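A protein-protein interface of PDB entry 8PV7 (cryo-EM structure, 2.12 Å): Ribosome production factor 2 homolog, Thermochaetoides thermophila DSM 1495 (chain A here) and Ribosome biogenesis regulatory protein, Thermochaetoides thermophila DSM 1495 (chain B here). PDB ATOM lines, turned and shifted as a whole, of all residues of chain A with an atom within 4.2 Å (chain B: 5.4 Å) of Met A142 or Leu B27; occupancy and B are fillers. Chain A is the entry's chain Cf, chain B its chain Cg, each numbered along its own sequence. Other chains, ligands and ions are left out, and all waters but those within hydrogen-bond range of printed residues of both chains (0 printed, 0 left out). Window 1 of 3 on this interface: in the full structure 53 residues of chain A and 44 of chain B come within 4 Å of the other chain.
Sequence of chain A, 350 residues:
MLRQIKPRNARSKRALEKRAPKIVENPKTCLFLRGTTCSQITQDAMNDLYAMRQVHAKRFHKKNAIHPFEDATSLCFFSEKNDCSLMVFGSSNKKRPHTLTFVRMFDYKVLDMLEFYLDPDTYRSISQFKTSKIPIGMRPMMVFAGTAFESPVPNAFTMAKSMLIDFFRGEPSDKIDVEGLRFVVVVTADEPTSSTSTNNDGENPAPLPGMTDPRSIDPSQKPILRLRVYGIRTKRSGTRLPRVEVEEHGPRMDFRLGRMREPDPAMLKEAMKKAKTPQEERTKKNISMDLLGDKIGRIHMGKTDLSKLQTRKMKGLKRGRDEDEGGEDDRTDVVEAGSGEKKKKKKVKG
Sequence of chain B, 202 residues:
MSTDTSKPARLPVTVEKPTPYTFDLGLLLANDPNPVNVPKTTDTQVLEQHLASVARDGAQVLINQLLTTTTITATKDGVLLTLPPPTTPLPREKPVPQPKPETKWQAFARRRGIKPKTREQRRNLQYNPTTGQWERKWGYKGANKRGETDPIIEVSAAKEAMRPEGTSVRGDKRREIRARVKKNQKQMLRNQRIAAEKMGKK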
ATOM      1  N   ARG A 139       0.256 -11.478 -20.811  1.00  0.00           N
ATOM      2  CA  ARG A 139      -1.049 -10.835 -20.847  1.00  0.00           C
ATOM      3  C   ARG A 139      -0.889  -9.338 -21.103  1.00  0.00           C
ATOM      4  O   ARG A 139      -0.037  -8.693 -20.492  1.00  0.00           O
ATOM      5  CB  ARG A 139      -1.808 -11.056 -19.540  1.00  0.00           C
ATOM      6  CG  ARG A 139      -0.962 -10.930 -18.295  1.00  0.00           C
ATOM      7  CD  ARG A 139      -1.627 -11.563 -17.093  1.00  0.00           C
ATOM      8  NE  ARG A 139      -2.696 -10.734 -16.555  1.00  0.00           N
ATOM      9  CZ  ARG A 139      -2.634 -10.092 -15.398  1.00  0.00           C
ATOM     10  NH1 ARG A 139      -1.564 -10.162 -14.625  1.00  0.00           N
ATOM     11  NH2 ARG A 139      -3.673  -9.362 -15.004  1.00  0.00           N
ATOM     12  N   PRO A 140      -1.670  -8.769 -22.010  1.00  0.00           N
ATOM     13  CA  PRO A 140      -1.638  -7.324 -22.227  1.00  0.00           C
ATOM     14  C   PRO A 140      -2.519  -6.604 -21.212  1.00  0.00           C
ATOM     15  O   PRO A 140      -3.313  -7.214 -20.496  1.00  0.00           O
ATOM     16  CB  PRO A 140      -2.208  -7.186 -23.640  1.00  0.00           C
ATOM     17  CG  PRO A 140      -3.190  -8.293 -23.722  1.00  0.00           C
ATOM     18  CD  PRO A 140      -2.657  -9.427 -22.882  1.00  0.00           C
ATOM     19  N   MET A 141      -2.356  -5.290 -21.157  1.00  0.00           N
ATOM     20  CA  MET A 141      -3.335  -4.481 -20.448  1.00  0.00           C
ATOM     21  C   MET A 141      -4.499  -4.160 -21.375  1.00  0.00           C
ATOM     22  O   MET A 141      -4.417  -4.337 -22.588  1.00  0.00           O
ATOM     23  CB  MET A 141      -2.708  -3.206 -19.890  1.00  0.00           C
ATOM     24  CG  MET A 141      -1.392  -3.442 -19.181  1.00  0.00           C
ATOM     25  SD  MET A 141      -0.568  -1.926 -18.678  1.00  0.00           S
ATOM     26  CE  MET A 141      -0.024  -1.307 -20.247  1.00  0.00           C
ATOM     27  N   MET A 142      -5.605  -3.717 -20.787  1.00  0.00           N
ATOM     28  CA  MET A 142      -6.828  -3.474 -21.538  1.00  0.00           C
ATOM     29  C   MET A 142      -7.319  -2.052 -21.326  1.00  0.00           C
ATOM     30  O   MET A 142      -7.294  -1.533 -20.207  1.00  0.00           O
ATOM     31  CB  MET A 142      -7.943  -4.457 -21.150  1.00  0.00           C
ATOM     32  CG  MET A 142      -7.964  -5.747 -21.946  1.00  0.00           C
ATOM     33  SD  MET A 142      -8.431  -7.194 -20.980  1.00  0.00           S
ATOM     34  CE  MET A 142      -7.161  -7.191 -19.731  1.00  0.00           C
ATOM     35  N   VAL A 143      -7.770  -1.429 -22.411  1.00  0.00           N
ATOM     36  CA  VAL A 143      -8.431  -0.132 -22.371  1.00  0.00           C
ATOM     37  C   VAL A 143      -9.747  -0.264 -23.123  1.00  0.00           C
ATOM     38  O   VAL A 143      -9.759  -0.669 -24.291  1.00  0.00           O
ATOM     39  CB  VAL A 143      -7.565   0.981 -22.985  1.00  0.00           C
ATOM     40  CG1 VAL A 143      -8.388   2.242 -23.195  1.00  0.00           C
ATOM     41  CG2 VAL A 143      -6.367   1.276 -22.102  1.00  0.00           C
ATOM     42  N   ILE A 165     -13.050  -9.016 -22.043  1.00  0.00           N
ATOM     43  CA  ILE A 165     -12.269  -9.082 -20.813  1.00  0.00           C
ATOM     44  C   ILE A 165     -11.958 -10.531 -20.461  1.00  0.00           C
ATOM     45  O   ILE A 165     -10.818 -10.869 -20.122  1.00  0.00           O
ATOM     46  CB  ILE A 165     -13.013  -8.363 -19.671  1.00  0.00           C
ATOM     47  CG1 ILE A 165     -12.936  -6.850 -19.851  1.00  0.00           C
ATOM     48  CG2 ILE A 165     -12.433  -8.729 -18.320  1.00  0.00           C
ATOM     49  CD1 ILE A 165     -13.879  -6.096 -18.954  1.00  0.00           C
ATOM     50  N   PHE A 168      -9.170 -11.740 -23.032  1.00  0.00           N
ATOM     51  CA  PHE A 168      -7.826 -11.207 -22.850  1.00  0.00           C
ATOM     52  C   PHE A 168      -7.386 -11.186 -21.393  1.00  0.00           C
ATOM     53  O   PHE A 168      -6.388 -10.536 -21.073  1.00  0.00           O
ATOM     54  CB  PHE A 168      -7.723  -9.798 -23.432  1.00  0.00           C
ATOM     55  CG  PHE A 168      -7.843  -9.744 -24.922  1.00  0.00           C
ATOM     56  CD1 PHE A 168      -6.810 -10.187 -25.729  1.00  0.00           C
ATOM     57  CD2 PHE A 168      -8.981  -9.235 -25.518  1.00  0.00           C
ATOM     58  CE1 PHE A 168      -6.914 -10.136 -27.103  1.00  0.00           C
ATOM     59  CE2 PHE A 168      -9.092  -9.180 -26.890  1.00  0.00           C
ATOM     60  CZ  PHE A 168      -8.057  -9.630 -27.685  1.00  0.00           C
ATOM     61  N   ARG A 169      -8.115 -11.868 -20.509  1.00  0.00           N
ATOM     62  CA  ARG A 169      -7.826 -11.818 -19.078  1.00  0.00           C
ATOM     63  C   ARG A 169      -6.477 -12.446 -18.742  1.00  0.00           C
ATOM     64  O   ARG A 169      -5.714 -11.902 -17.936  1.00  0.00           O
ATOM     65  CB  ARG A 169      -8.947 -12.519 -18.316  1.00  0.00           C
ATOM     66  CG  ARG A 169      -9.057 -12.167 -16.862  1.00  0.00           C
ATOM     67  CD  ARG A 169      -9.959 -13.162 -16.155  1.00  0.00           C
ATOM     68  NE  ARG A 169     -10.183 -12.813 -14.758  1.00  0.00           N
ATOM     69  CZ  ARG A 169      -9.310 -13.019 -13.784  1.00  0.00           C
ATOM     70  NH1 ARG A 169      -8.133 -13.576 -14.016  1.00  0.00           N
ATOM     71  NH2 ARG A 169      -9.623 -12.655 -12.544  1.00  0.00           N
ATOM     72  N   VAL A 185      -4.369  -3.797 -25.383  1.00  0.00           N
ATOM     73  CA  VAL A 185      -5.495  -4.032 -26.273  1.00  0.00           C
ATOM     74  C   VAL A 185      -6.535  -2.954 -26.008  1.00  0.00           C
ATOM     75  O   VAL A 185      -6.968  -2.769 -24.863  1.00  0.00           O
ATOM     76  CB  VAL A 185      -6.089  -5.433 -26.050  1.00  0.00           C
ATOM     77  CG1 VAL A 185      -7.331  -5.613 -26.882  1.00  0.00           C
ATOM     78  CG2 VAL A 185      -5.066  -6.505 -26.373  1.00  0.00           C
ATOM     79  N   ASP B  24      -9.336  -1.100 -12.932  1.00  0.00           N
ATOM     80  CA  ASP B  24      -9.298  -2.386 -12.241  1.00  0.00           C
ATOM     81  C   ASP B  24      -7.865  -2.876 -12.452  1.00  0.00           C
ATOM     82  O   ASP B  24      -7.539  -3.504 -13.460  1.00  0.00           O
ATOM     83  CB  ASP B  24     -10.337  -3.368 -12.780  1.00  0.00           C
ATOM     84  CG  ASP B  24     -10.474  -4.610 -11.917  1.00  0.00           C
ATOM     85  OD1 ASP B  24     -11.449  -5.355 -12.115  1.00  0.00           O
ATOM     86  OD2 ASP B  24      -9.633  -4.844 -11.027  1.00  0.00           O
ATOM     87  N   LEU B  25      -6.994  -2.558 -11.495  1.00  0.00           N
ATOM     88  CA  LEU B  25      -5.581  -2.870 -11.657  1.00  0.00           C
ATOM     89  C   LEU B  25      -5.297  -4.357 -11.500  1.00  0.00           C
ATOM     90  O   LEU B  25      -4.230  -4.817 -11.913  1.00  0.00           O
ATOM     91  CB  LEU B  25      -4.750  -2.062 -10.663  1.00  0.00           C
ATOM     92  CG  LEU B  25      -4.921  -0.544 -10.728  1.00  0.00           C
ATOM     93  CD1 LEU B  25      -3.924   0.140  -9.818  1.00  0.00           C
ATOM     94  CD2 LEU B  25      -4.784  -0.029 -12.150  1.00  0.00           C
ATOM     95  N   GLY B  26      -6.222  -5.112 -10.907  1.00  0.00           N
ATOM     96  CA  GLY B  26      -6.084  -6.556 -10.886  1.00  0.00           C
ATOM     97  C   GLY B  26      -6.144  -7.170 -12.268  1.00  0.00           C
ATOM     98  O   GLY B  26      -5.469  -8.164 -12.540  1.00  0.00           O
ATOM     99  N   LEU B  27      -6.949  -6.592 -13.156  1.00  0.00           N
ATOM    100  CA  LEU B  27      -7.051  -7.036 -14.537  1.00  0.00           C
ATOM    101  C   LEU B  27      -6.226  -6.186 -15.490  1.00  0.00           C
ATOM    102  O   LEU B  27      -6.275  -6.423 -16.699  1.00  0.00           O
ATOM    103  CB  LEU B  27      -8.513  -7.033 -14.981  1.00  0.00           C
ATOM    104  CG  LEU B  27      -9.473  -7.895 -14.170  1.00  0.00           C
ATOM    105  CD1 LEU B  27     -10.884  -7.734 -14.688  1.00  0.00           C
ATOM    106  CD2 LEU B  27      -9.050  -9.346 -14.221  1.00  0.00           C
ATOM    107  N   LEU B  28      -5.475  -5.208 -14.970  1.00  0.00           N
ATOM    108  CA  LEU B  28      -4.746  -4.217 -15.770  1.00  0.00           C
ATOM    109  C   LEU B  28      -5.677  -3.494 -16.738  1.00  0.00           C
ATOM    110  O   LEU B  28      -5.338  -3.251 -17.896  1.00  0.00           O
ATOM    111  CB  LEU B  28      -3.572  -4.850 -16.518  1.00  0.00           C
ATOM    112  CG  LEU B  28      -2.620  -5.720 -15.703  1.00  0.00           C
ATOM    113  CD1 LEU B  28      -1.735  -6.523 -16.628  1.00  0.00           C
ATOM    114  CD2 LEU B  28      -1.785  -4.850 -14.790  1.00  0.00           C
ATOM    115  N   LEU B  29      -6.868  -3.148 -16.259  1.00  0.00           N
ATOM    116  CA  LEU B  29      -7.942  -2.630 -17.090  1.00  0.00           C
ATOM    117  C   LEU B  29      -8.185  -1.159 -16.781  1.00  0.00           C
ATOM    118  O   LEU B  29      -8.309  -0.777 -15.614  1.00  0.00           O
ATOM    119  CB  LEU B  29      -9.220  -3.438 -16.865  1.00  0.00           C
ATOM    120  CG  LEU B  29     -10.527  -2.875 -17.411  1.00  0.00           C
ATOM    121  CD1 LEU B  29     -10.451  -2.773 -18.910  1.00  0.00           C
ATOM    122  CD2 LEU B  29     -11.682  -3.758 -16.998  1.00  0.00           C
ATOM    123  N   ALA B  30      -8.256  -0.343 -17.827  1.00  0.00           N
ATOM    124  CA  ALA B  30      -8.631   1.058 -17.715  1.00  0.00           C
ATOM    125  C   ALA B  30      -9.902   1.292 -18.514  1.00  0.00           C
ATOM    126  O   ALA B  30      -9.966   0.951 -19.698  1.00  0.00           O
ATOM    127  CB  ALA B  30      -7.513   1.975 -18.213  1.00  0.00           C
ATOM    128  N   LEU B  62      -3.080   4.482 -17.504  1.00  0.00           N
ATOM    129  CA  LEU B  62      -2.923   3.167 -16.888  1.00  0.00           C
ATOM    130  C   LEU B  62      -1.537   3.009 -16.272  1.00  0.00           C
ATOM    131  O   LEU B  62      -1.401   2.541 -15.134  1.00  0.00           O
ATOM    132  CB  LEU B  62      -3.188   2.075 -17.923  1.00  0.00           C
ATOM    133  CG  LEU B  62      -3.528   0.666 -17.435  1.00  0.00           C
ATOM    134  CD1 LEU B  62      -4.280   0.690 -16.115  1.00  0.00           C
ATOM    135  CD2 LEU B  62      -4.329  -0.062 -18.495  1.00  0.00           C
ATOM    136  N   PRO B  86      -8.934  -8.522  -8.365  1.00  0.00           N
ATOM    137  CA  PRO B  86      -9.823  -7.970  -9.397  1.00  0.00           C
ATOM    138  C   PRO B  86     -11.224  -7.707  -8.867  1.00  0.00           C
ATOM    139  O   PRO B  86     -11.760  -8.471  -8.062  1.00  0.00           O
ATOM    140  CB  PRO B  86      -9.829  -9.060 -10.476  1.00  0.00           C
ATOM    141  CG  PRO B  86      -8.593  -9.853 -10.225  1.00  0.00           C
ATOM    142  CD  PRO B  86      -8.407  -9.842  -8.744  1.00  0.00           C
ATOM    143  N   THR B  88     -13.844  -6.337 -11.205  1.00  0.00           N
ATOM    144  CA  THR B  88     -14.837  -6.416 -12.269  1.00  0.00           C
ATOM    145  C   THR B  88     -15.574  -7.746 -12.186  1.00  0.00           C
ATOM    146  O   THR B  88     -14.929  -8.804 -12.207  1.00  0.00           O
ATOM    147  CB  THR B  88     -14.187  -6.267 -13.639  1.00  0.00           C
ATOM    148  OG1 THR B  88     -13.615  -4.960 -13.757  1.00  0.00           O
ATOM    149  CG2 THR B  88     -15.210  -6.464 -14.741  1.00  0.00           C
ATOM    150  N   LEU B  90     -17.177 -11.022 -13.207  1.00  0.00           N
ATOM    151  CA  LEU B  90     -17.100 -11.911 -14.352  1.00  0.00           C
ATOM    152  C   LEU B  90     -17.710 -13.246 -13.965  1.00  0.00           C
ATOM    153  O   LEU B  90     -17.597 -13.667 -12.808  1.00  0.00           O
ATOM    154  CB  LEU B  90     -15.648 -12.114 -14.814  1.00  0.00           C
ATOM    155  CG  LEU B  90     -14.970 -10.910 -15.468  1.00  0.00           C
ATOM    156  CD1 LEU B  90     -13.468 -11.104 -15.500  1.00  0.00           C
ATOM    157  CD2 LEU B  90     -15.508 -10.683 -16.869  1.00  0.00           C
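N of Met A142 is in hydrogen-bond range of O of Leu B28, 2.9 Å away. O of Met A142 is in hydrogen-bond range of N of Ala B30, at 2.8 Å. The backbone carbonyl oxygen (O) of Gly B26 sits at hydrogen-bond distance from the guanidinium group (NH2) of Arg A139, 3.3 Å away.
The backbone NH of Asp B24 lies within hydrogen-bond range of the backbone carbonyl oxygen of Leu B29, 2.9 Å away. O of Met A141 lies within hydrogen-bond range of N of Val A185, 2.8 Å away. N of Val A143 lies within hydrogen-bond range of O of Val A185 (2.9 Å). The side-chain carboxylate of Asp B24 lies close to the backbone NH of Gly B26.
Among the printed residues, merely in contact across the chains: Met A142 with Leu B27, Val A143 with Ala B30, Met A141 with Leu B28, Met A142 with Leu B29, Arg A169 with Leu B27, Met A142 with Leu B62, Ile A165 with Leu B29, Arg A169 with Leu B90, Arg A169 with Pro B86, Arg A139 with Leu B28, Met A141 with Leu B62 and Ile A165 with Leu B90.
Met A142 touches five residues of chain B. Of chain A, only Met A142 (3.3 Å) and Arg A169 (3.7 Å) come within 4 Å of Leu B27. Of the printed residues of chain A, Leu B28 touches Arg A139, Met A141 and Met A142. Of the printed residues of chain B, Met A141 touches Leu B28 (3.3 Å) and Leu B62 (3.8 Å). Of the printed residues of chain A, Leu B62 touches Met A141 and Met A142. Of the printed residues of chain A, Leu B90 touches Ile A165 and Arg A169. Printed residues of chain A within 4 Å of Leu B29: Met A142 and Ile A165. Pro A140 touches none of the printed residues of chain B. Phe A168 touches none of the printed residues of chain B. The nearest printed residue of chain B that does not touch Met A142 is Asp B24 (7.0 Å).
Of the 11 printed residues of chain B, 8 touch a printed residue of chain A. Of the 9 printed residues of chain A, 6 touch a printed residue of chain B. Hydrophobic or aromatic side chains of chain A within 4 Å of the printed part of chain B: Met A141, Met A142 and Ile A165. Along chain A the printed residues that touch a printed residue of chain B span positions 139 to 169. Among the printed residues, no Asp or Glu carboxylate lies within 4 Å of a Lys or Arg side-chain nitrogen of the other chain.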
